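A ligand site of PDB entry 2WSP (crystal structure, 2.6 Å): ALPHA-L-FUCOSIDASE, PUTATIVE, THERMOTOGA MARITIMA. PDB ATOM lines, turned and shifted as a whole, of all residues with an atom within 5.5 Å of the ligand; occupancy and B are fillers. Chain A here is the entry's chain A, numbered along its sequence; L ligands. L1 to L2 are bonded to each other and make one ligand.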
ATOM      1  N   PHE A  32      22.756 -16.778 -20.429  1.00  0.00           N
ATOM      2  CA  PHE A  32      21.773 -17.167 -19.428  1.00  0.00           C
ATOM      3  C   PHE A  32      21.403 -18.614 -19.757  1.00  0.00           C
ATOM      4  O   PHE A  32      21.330 -18.956 -20.936  1.00  0.00           O
ATOM      5  CB  PHE A  32      20.531 -16.274 -19.596  1.00  0.00           C
ATOM      6  CG  PHE A  32      19.880 -15.818 -18.313  1.00  0.00           C
ATOM      7  CD1 PHE A  32      20.028 -16.487 -17.110  1.00  0.00           C
ATOM      8  CD2 PHE A  32      19.050 -14.700 -18.337  1.00  0.00           C
ATOM      9  CE1 PHE A  32      19.388 -16.032 -15.957  1.00  0.00           C
ATOM     10  CE2 PHE A  32      18.421 -14.243 -17.193  1.00  0.00           C
ATOM     11  CZ  PHE A  32      18.591 -14.909 -16.008  1.00  0.00           C
ATOM     12  N   HIS A  34      18.213 -21.155 -18.799  1.00  0.00           N
ATOM     13  CA  HIS A  34      17.008 -21.631 -18.137  1.00  0.00           C
ATOM     14  C   HIS A  34      16.829 -23.103 -18.451  1.00  0.00           C
ATOM     15  O   HIS A  34      16.429 -23.478 -19.551  1.00  0.00           O
ATOM     16  CB  HIS A  34      15.780 -20.840 -18.583  1.00  0.00           C
ATOM     17  CG  HIS A  34      15.675 -19.492 -17.941  1.00  0.00           C
ATOM     18  ND1 HIS A  34      16.587 -18.485 -18.179  1.00  0.00           N
ATOM     19  CD2 HIS A  34      14.767 -18.980 -17.080  1.00  0.00           C
ATOM     20  CE1 HIS A  34      16.237 -17.412 -17.499  1.00  0.00           C
ATOM     21  NE2 HIS A  34      15.135 -17.679 -16.822  1.00  0.00           N
ATOM     22  N   LEU A  50       7.119  -9.267 -24.606  1.00  0.00           N
ATOM     23  CA  LEU A  50       6.572  -8.265 -23.697  1.00  0.00           C
ATOM     24  C   LEU A  50       6.301  -6.962 -24.453  1.00  0.00           C
ATOM     25  O   LEU A  50       7.169  -6.470 -25.184  1.00  0.00           O
ATOM     26  CB  LEU A  50       7.527  -8.000 -22.525  1.00  0.00           C
ATOM     27  CG  LEU A  50       7.602  -9.052 -21.406  1.00  0.00           C
ATOM     28  CD1 LEU A  50       8.935  -8.957 -20.675  1.00  0.00           C
ATOM     29  CD2 LEU A  50       6.432  -8.931 -20.436  1.00  0.00           C
ATOM     30  N   MET A  55      -1.134  -8.096 -21.963  1.00  0.00           N
ATOM     31  CA  MET A  55      -0.759  -8.593 -20.637  1.00  0.00           C
ATOM     32  C   MET A  55      -1.951  -9.147 -19.838  1.00  0.00           C
ATOM     33  O   MET A  55      -1.773  -9.764 -18.780  1.00  0.00           O
ATOM     34  CB  MET A  55      -0.066  -7.482 -19.830  1.00  0.00           C
ATOM     35  CG  MET A  55       0.908  -7.982 -18.761  1.00  0.00           C
ATOM     36  SD  MET A  55       2.420  -8.686 -19.461  1.00  0.00           S
ATOM     37  CE  MET A  55       3.254  -9.295 -17.991  1.00  0.00           C
ATOM     38  N   TRP A  58      -1.655 -12.806 -21.033  1.00  0.00           N
ATOM     39  CA  TRP A  58      -0.278 -13.327 -20.997  1.00  0.00           C
ATOM     40  C   TRP A  58      -0.128 -14.641 -20.233  1.00  0.00           C
ATOM     41  O   TRP A  58       0.457 -15.584 -20.741  1.00  0.00           O
ATOM     42  CB  TRP A  58       0.663 -12.270 -20.413  1.00  0.00           C
ATOM     43  CG  TRP A  58       2.097 -12.721 -20.296  1.00  0.00           C
ATOM     44  CD1 TRP A  58       2.681 -13.364 -19.243  1.00  0.00           C
ATOM     45  CD2 TRP A  58       3.136 -12.561 -21.278  1.00  0.00           C
ATOM     46  NE1 TRP A  58       4.005 -13.619 -19.504  1.00  0.00           N
ATOM     47  CE2 TRP A  58       4.308 -13.130 -20.750  1.00  0.00           C
ATOM     48  CE3 TRP A  58       3.184 -11.991 -22.561  1.00  0.00           C
ATOM     49  CZ2 TRP A  58       5.524 -13.144 -21.447  1.00  0.00           C
ATOM     50  CZ3 TRP A  58       4.381 -12.006 -23.259  1.00  0.00           C
ATOM     51  CH2 TRP A  58       5.541 -12.579 -22.703  1.00  0.00           C
ATOM     52  N   PHE A  59      -0.645 -14.693 -19.004  1.00  0.00           N
ATOM     53  CA  PHE A  59      -0.473 -15.869 -18.168  1.00  0.00           C
ATOM     54  C   PHE A  59      -1.335 -17.037 -18.632  1.00  0.00           C
ATOM     55  O   PHE A  59      -0.997 -18.202 -18.384  1.00  0.00           O
ATOM     56  CB  PHE A  59      -0.759 -15.546 -16.701  1.00  0.00           C
ATOM     57  CG  PHE A  59       0.174 -14.510 -16.129  1.00  0.00           C
ATOM     58  CD1 PHE A  59       1.489 -14.842 -15.813  1.00  0.00           C
ATOM     59  CD2 PHE A  59      -0.238 -13.199 -15.940  1.00  0.00           C
ATOM     60  CE1 PHE A  59       2.364 -13.887 -15.303  1.00  0.00           C
ATOM     61  CE2 PHE A  59       0.627 -12.244 -15.431  1.00  0.00           C
ATOM     62  CZ  PHE A  59       1.923 -12.589 -15.108  1.00  0.00           C
ATOM     63  N   ASN A  62       0.788 -18.244 -21.951  1.00  0.00           N
ATOM     64  CA  ASN A  62       2.154 -17.862 -21.579  1.00  0.00           C
ATOM     65  C   ASN A  62       3.222 -18.396 -22.518  1.00  0.00           C
ATOM     66  O   ASN A  62       3.370 -19.611 -22.663  1.00  0.00           O
ATOM     67  CB  ASN A  62       2.445 -18.313 -20.146  1.00  0.00           C
ATOM     68  CG  ASN A  62       3.570 -17.517 -19.493  1.00  0.00           C
ATOM     69  OD1 ASN A  62       4.517 -17.093 -20.153  1.00  0.00           O
ATOM     70  ND2 ASN A  62       3.459 -17.309 -18.190  1.00  0.00           N
ATOM     71  N   TYR A  64       6.418 -18.209 -22.055  1.00  0.00           N
ATOM     72  CA  TYR A  64       7.588 -18.654 -21.287  1.00  0.00           C
ATOM     73  C   TYR A  64       7.354 -20.090 -20.839  1.00  0.00           C
ATOM     74  O   TYR A  64       6.471 -20.357 -20.031  1.00  0.00           O
ATOM     75  CB  TYR A  64       7.794 -17.740 -20.075  1.00  0.00           C
ATOM     76  CG  TYR A  64       8.278 -16.333 -20.373  1.00  0.00           C
ATOM     77  CD1 TYR A  64       8.605 -15.457 -19.343  1.00  0.00           C
ATOM     78  CD2 TYR A  64       8.407 -15.854 -21.685  1.00  0.00           C
ATOM     79  CE1 TYR A  64       9.032 -14.158 -19.593  1.00  0.00           C
ATOM     80  CE2 TYR A  64       8.836 -14.565 -21.946  1.00  0.00           C
ATOM     81  CZ  TYR A  64       9.154 -13.721 -20.900  1.00  0.00           C
ATOM     82  OH  TYR A  64       9.581 -12.433 -21.141  1.00  0.00           O
ATOM     83  N   GLU A  66       9.180 -22.043 -19.074  1.00  0.00           N
ATOM     84  CA  GLU A  66       9.527 -22.287 -17.661  1.00  0.00           C
ATOM     85  C   GLU A  66       8.307 -22.106 -16.751  1.00  0.00           C
ATOM     86  O   GLU A  66       8.292 -22.631 -15.643  1.00  0.00           O
ATOM     87  CB  GLU A  66      10.645 -21.372 -17.142  1.00  0.00           C
ATOM     88  CG  GLU A  66      11.496 -20.671 -18.172  1.00  0.00           C
ATOM     89  CD  GLU A  66      10.826 -19.415 -18.715  1.00  0.00           C
ATOM     90  OE1 GLU A  66      10.791 -18.398 -18.010  1.00  0.00           O
ATOM     91  OE2 GLU A  66      10.355 -19.460 -19.858  1.00  0.00           O
ATOM     92  N   TRP A  67       7.324 -21.334 -17.207  1.00  0.00           N
ATOM     93  CA  TRP A  67       6.078 -21.124 -16.468  1.00  0.00           C
ATOM     94  C   TRP A  67       5.060 -22.267 -16.592  1.00  0.00           C
ATOM     95  O   TRP A  67       3.944 -22.152 -16.081  1.00  0.00           O
ATOM     96  CB  TRP A  67       5.441 -19.792 -16.892  1.00  0.00           C
ATOM     97  CG  TRP A  67       6.116 -18.631 -16.244  1.00  0.00           C
ATOM     98  CD1 TRP A  67       7.394 -18.198 -16.470  1.00  0.00           C
ATOM     99  CD2 TRP A  67       5.571 -17.787 -15.236  1.00  0.00           C
ATOM    100  NE1 TRP A  67       7.667 -17.131 -15.664  1.00  0.00           N
ATOM    101  CE2 TRP A  67       6.574 -16.861 -14.887  1.00  0.00           C
ATOM    102  CE3 TRP A  67       4.334 -17.722 -14.577  1.00  0.00           C
ATOM    103  CZ2 TRP A  67       6.365 -15.865 -13.928  1.00  0.00           C
ATOM    104  CZ3 TRP A  67       4.137 -16.734 -13.628  1.00  0.00           C
ATOM    105  CH2 TRP A  67       5.144 -15.816 -13.309  1.00  0.00           C
ATOM    106  N   HIS A 128      14.410 -22.058 -10.238  1.00  0.00           N
ATOM    107  CA  HIS A 128      13.459 -21.144 -10.832  1.00  0.00           C
ATOM    108  C   HIS A 128      12.160 -21.135 -10.002  1.00  0.00           C
ATOM    109  O   HIS A 128      12.161 -21.553  -8.834  1.00  0.00           O
ATOM    110  CB  HIS A 128      13.207 -21.543 -12.292  1.00  0.00           C
ATOM    111  CG  HIS A 128      12.738 -20.410 -13.149  1.00  0.00           C
ATOM    112  ND1 HIS A 128      11.426 -20.283 -13.550  1.00  0.00           N
ATOM    113  CD2 HIS A 128      13.394 -19.319 -13.625  1.00  0.00           C
ATOM    114  CE1 HIS A 128      11.296 -19.173 -14.246  1.00  0.00           C
ATOM    115  NE2 HIS A 128      12.476 -18.577 -14.318  1.00  0.00           N
ATOM    116  N   HIS A 129      11.068 -20.637 -10.567  1.00  0.00           N
ATOM    117  CA  HIS A 129       9.826 -20.466  -9.842  1.00  0.00           C
ATOM    118  C   HIS A 129       9.217 -21.785  -9.358  1.00  0.00           C
ATOM    119  O   HIS A 129       8.604 -21.825  -8.288  1.00  0.00           O
ATOM    120  CB  HIS A 129       8.798 -19.693 -10.674  1.00  0.00           C
ATOM    121  CG  HIS A 129       9.316 -18.397 -11.238  1.00  0.00           C
ATOM    122  ND1 HIS A 129      10.332 -17.688 -10.632  1.00  0.00           N
ATOM    123  CD2 HIS A 129       8.953 -17.693 -12.327  1.00  0.00           C
ATOM    124  CE1 HIS A 129      10.577 -16.596 -11.336  1.00  0.00           C
ATOM    125  NE2 HIS A 129       9.748 -16.578 -12.376  1.00  0.00           N
ATOM    126  N   TYR A 171      21.705 -17.842 -11.118  1.00  0.00           N
ATOM    127  CA  TYR A 171      20.339 -17.338 -11.043  1.00  0.00           C
ATOM    128  C   TYR A 171      19.594 -18.076  -9.926  1.00  0.00           C
ATOM    129  O   TYR A 171      19.632 -19.304  -9.860  1.00  0.00           O
ATOM    130  CB  TYR A 171      19.593 -17.526 -12.362  1.00  0.00           C
ATOM    131  CG  TYR A 171      18.116 -17.183 -12.259  1.00  0.00           C
ATOM    132  CD1 TYR A 171      17.200 -18.097 -11.744  1.00  0.00           C
ATOM    133  CD2 TYR A 171      17.652 -15.931 -12.633  1.00  0.00           C
ATOM    134  CE1 TYR A 171      15.864 -17.775 -11.619  1.00  0.00           C
ATOM    135  CE2 TYR A 171      16.305 -15.598 -12.519  1.00  0.00           C
ATOM    136  CZ  TYR A 171      15.422 -16.529 -12.012  1.00  0.00           C
ATOM    137  OH  TYR A 171      14.077 -16.227 -11.890  1.00  0.00           O
ATOM    138  N   TRP A 222      22.318 -13.381  -9.340  1.00  0.00           N
ATOM    139  CA  TRP A 222      21.241 -12.862 -10.195  1.00  0.00           C
ATOM    140  C   TRP A 222      19.906 -13.342  -9.645  1.00  0.00           C
ATOM    141  O   TRP A 222      19.510 -14.477  -9.854  1.00  0.00           O
ATOM    142  CB  TRP A 222      21.429 -13.388 -11.625  1.00  0.00           C
ATOM    143  CG  TRP A 222      20.962 -12.479 -12.739  1.00  0.00           C
ATOM    144  CD1 TRP A 222      21.755 -11.764 -13.603  1.00  0.00           C
ATOM    145  CD2 TRP A 222      19.611 -12.224 -13.145  1.00  0.00           C
ATOM    146  NE1 TRP A 222      20.971 -11.077 -14.499  1.00  0.00           N
ATOM    147  CE2 TRP A 222      19.658 -11.344 -14.244  1.00  0.00           C
ATOM    148  CE3 TRP A 222      18.360 -12.661 -12.675  1.00  0.00           C
ATOM    149  CZ2 TRP A 222      18.505 -10.886 -14.889  1.00  0.00           C
ATOM    150  CZ3 TRP A 222      17.207 -12.203 -13.319  1.00  0.00           C
ATOM    151  CH2 TRP A 222      17.294 -11.320 -14.415  1.00  0.00           C
ATOM    152  N   MET A 225      12.433 -11.895  -9.479  1.00  0.00           N
ATOM    153  CA  MET A 225      11.110 -11.651  -8.906  1.00  0.00           C
ATOM    154  C   MET A 225      11.130 -11.057  -7.493  1.00  0.00           C
ATOM    155  O   MET A 225      10.184 -11.247  -6.716  1.00  0.00           O
ATOM    156  CB  MET A 225      10.257 -12.936  -8.956  1.00  0.00           C
ATOM    157  CG  MET A 225       9.902 -13.366 -10.368  1.00  0.00           C
ATOM    158  SD  MET A 225       8.770 -12.202 -11.171  1.00  0.00           S
ATOM    159  CE  MET A 225       7.361 -12.281 -10.065  1.00  0.00           C
ATOM    160  N   ARG A 254      17.207  -6.929  -8.740  1.00  0.00           N
ATOM    161  CA  ARG A 254      15.868  -7.481  -8.619  1.00  0.00           C
ATOM    162  C   ARG A 254      15.654  -8.101  -7.243  1.00  0.00           C
ATOM    163  O   ARG A 254      15.006  -9.139  -7.115  1.00  0.00           O
ATOM    164  CB  ARG A 254      15.651  -8.514  -9.720  1.00  0.00           C
ATOM    165  CG  ARG A 254      15.780  -7.929 -11.125  1.00  0.00           C
ATOM    166  CD  ARG A 254      15.239  -8.913 -12.151  1.00  0.00           C
ATOM    167  NE  ARG A 254      15.361  -8.402 -13.523  1.00  0.00           N
ATOM    168  CZ  ARG A 254      14.703  -8.881 -14.573  1.00  0.00           C
ATOM    169  NH1 ARG A 254      13.854  -9.905 -14.452  1.00  0.00           N
ATOM    170  NH2 ARG A 254      14.896  -8.345 -15.765  1.00  0.00           N
ATOM    171  N   GLU A 266      14.481  -5.799 -19.585  1.00  0.00           N
ATOM    172  CA  GLU A 266      13.862  -6.845 -20.380  1.00  0.00           C
ATOM    173  C   GLU A 266      12.910  -6.263 -21.431  1.00  0.00           C
ATOM    174  O   GLU A 266      11.942  -6.911 -21.847  1.00  0.00           O
ATOM    175  CB  GLU A 266      13.189  -7.886 -19.459  1.00  0.00           C
ATOM    176  CG  GLU A 266      12.695  -7.352 -18.096  1.00  0.00           C
ATOM    177  CD  GLU A 266      11.393  -6.560 -18.186  1.00  0.00           C
ATOM    178  OE1 GLU A 266      11.265  -5.542 -17.460  1.00  0.00           O
ATOM    179  OE2 GLU A 266      10.491  -6.958 -18.961  1.00  0.00           O
ATOM    180  N   THR A 283      18.602  -8.580 -21.025  1.00  0.00           N
ATOM    181  CA  THR A 283      18.435 -10.030 -21.054  1.00  0.00           C
ATOM    182  C   THR A 283      17.272 -10.388 -21.990  1.00  0.00           C
ATOM    183  O   THR A 283      16.222  -9.765 -21.939  1.00  0.00           O
ATOM    184  CB  THR A 283      18.182 -10.595 -19.638  1.00  0.00           C
ATOM    185  OG1 THR A 283      18.313 -12.021 -19.649  1.00  0.00           O
ATOM    186  CG2 THR A 283      16.803 -10.222 -19.112  1.00  0.00           C
ATOM    187  N   PHE A 290      12.328 -18.408 -22.382  1.00  0.00           N
ATOM    188  CA  PHE A 290      13.641 -18.648 -21.798  1.00  0.00           C
ATOM    189  C   PHE A 290      13.911 -20.149 -21.722  1.00  0.00           C
ATOM    190  O   PHE A 290      14.990 -20.597 -22.100  1.00  0.00           O
ATOM    191  CB  PHE A 290      13.742 -18.015 -20.415  1.00  0.00           C
ATOM    192  CG  PHE A 290      13.770 -16.513 -20.444  1.00  0.00           C
ATOM    193  CD1 PHE A 290      12.592 -15.792 -20.518  1.00  0.00           C
ATOM    194  CD2 PHE A 290      14.972 -15.821 -20.407  1.00  0.00           C
ATOM    195  CE1 PHE A 290      12.608 -14.401 -20.547  1.00  0.00           C
ATOM    196  CE2 PHE A 290      14.999 -14.429 -20.444  1.00  0.00           C
ATOM    197  CZ  PHE A 290      13.812 -13.719 -20.510  1.00  0.00           C
HETATM  198  C1  LIG L   1       8.266 -11.622 -15.956  1.00  0.00           C
HETATM  199  N1  LIG L   1       7.879 -12.918 -15.390  1.00  0.00           N
HETATM  200  C2  LIG L   1       9.789 -11.484 -15.970  1.00  0.00           C
HETATM  201  N2  LIG L   1       7.233 -13.720 -16.100  1.00  0.00           N
HETATM  202  O1  LIG L   1      10.482 -12.667 -16.365  1.00  0.00           O
HETATM  203  C3  LIG L   1      10.072 -10.323 -16.917  1.00  0.00           C
HETATM  204  N3  LIG L   1       6.599 -14.479 -16.856  1.00  0.00           N
HETATM  205  O2  LIG L   1      11.487 -10.163 -17.100  1.00  0.00           O
HETATM  206  C4  LIG L   1       9.425  -9.057 -16.340  1.00  0.00           C
HETATM  207  O3  LIG L   1      10.189  -8.592 -15.231  1.00  0.00           O
HETATM  208  C5  LIG L   1       7.967  -9.269 -15.883  1.00  0.00           C
HETATM  209  O4  LIG L   1       7.776 -10.516 -15.195  1.00  0.00           O
HETATM  210  C6  LIG L   1       7.528  -8.117 -14.973  1.00  0.00           C
HETATM  211  C1  LG2 L   2      11.315 -13.237 -15.345  1.00  0.00           C
HETATM  212  C2  LG2 L   2      10.919 -14.695 -15.083  1.00  0.00           C
HETATM  213  C3  LG2 L   2      11.202 -15.537 -16.307  1.00  0.00           C
HETATM  214  C4  LG2 L   2      12.672 -15.429 -16.700  1.00  0.00           C
HETATM  215  C5  LG2 L   2      13.059 -13.958 -16.871  1.00  0.00           C
HETATM  216  C6  LG2 L   2      14.553 -13.838 -17.110  1.00  0.00           C
HETATM  217  O1  LG2 L   2       9.545 -14.823 -14.723  1.00  0.00           O
HETATM  218  O2  LG2 L   2      10.867 -16.891 -16.022  1.00  0.00           O
HETATM  219  O3  LG2 L   2      13.478 -16.031 -15.684  1.00  0.00           O
HETATM  220  O4  LG2 L   2      12.697 -13.177 -15.729  1.00  0.00           O
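O3 of LG2 L2 is in hydrogen-bond range of NE2 of His 34 (2.6 Å). An oxygen (O1) of LG2 L2 lies within hydrogen-bond range of the indole nitrogen (NE1) of Trp 67 (3.1 Å). O1 of LG2 L2 lies within hydrogen-bond range of NE2 of His 129. OE1 of Glu 66 lies within hydrogen-bond range of O2 of LG2 L2 (2.5 Å). NE2 of His 128 is in hydrogen-bond range of O2 of LG2 L2 (2.9 Å).
The side-chain carboxylate (OE2) of Glu 66 sits at hydrogen-bond distance from the backbone NH (N) of Phe 290, at 3.4 Å. N of Tyr 64 sits at hydrogen-bond distance from OD1 of Asn 62.
Phe 32 touches the ligand. NE1 of Trp 58 touches N3 of LIG L1 (3.8 Å). Tyr 64 touches the ligand. OH of Tyr 171 touches O3 of LG2 L2 (3.8 Å). NH1 of Arg 254 touches O2 of LIG L1 (3.6 Å). Glu 266 touches the ligand. CE2 of Phe 290 touches C6 of LG2 L2 (3.4 Å). Hydrophobic or aromatic side chains within 4 Å of the ligand: Phe 32, His 34, Tyr 64, Trp 67, His 128, His 129 and Phe 290. Of the 19 residues printed, 12 come within 4 Å of the ligand.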
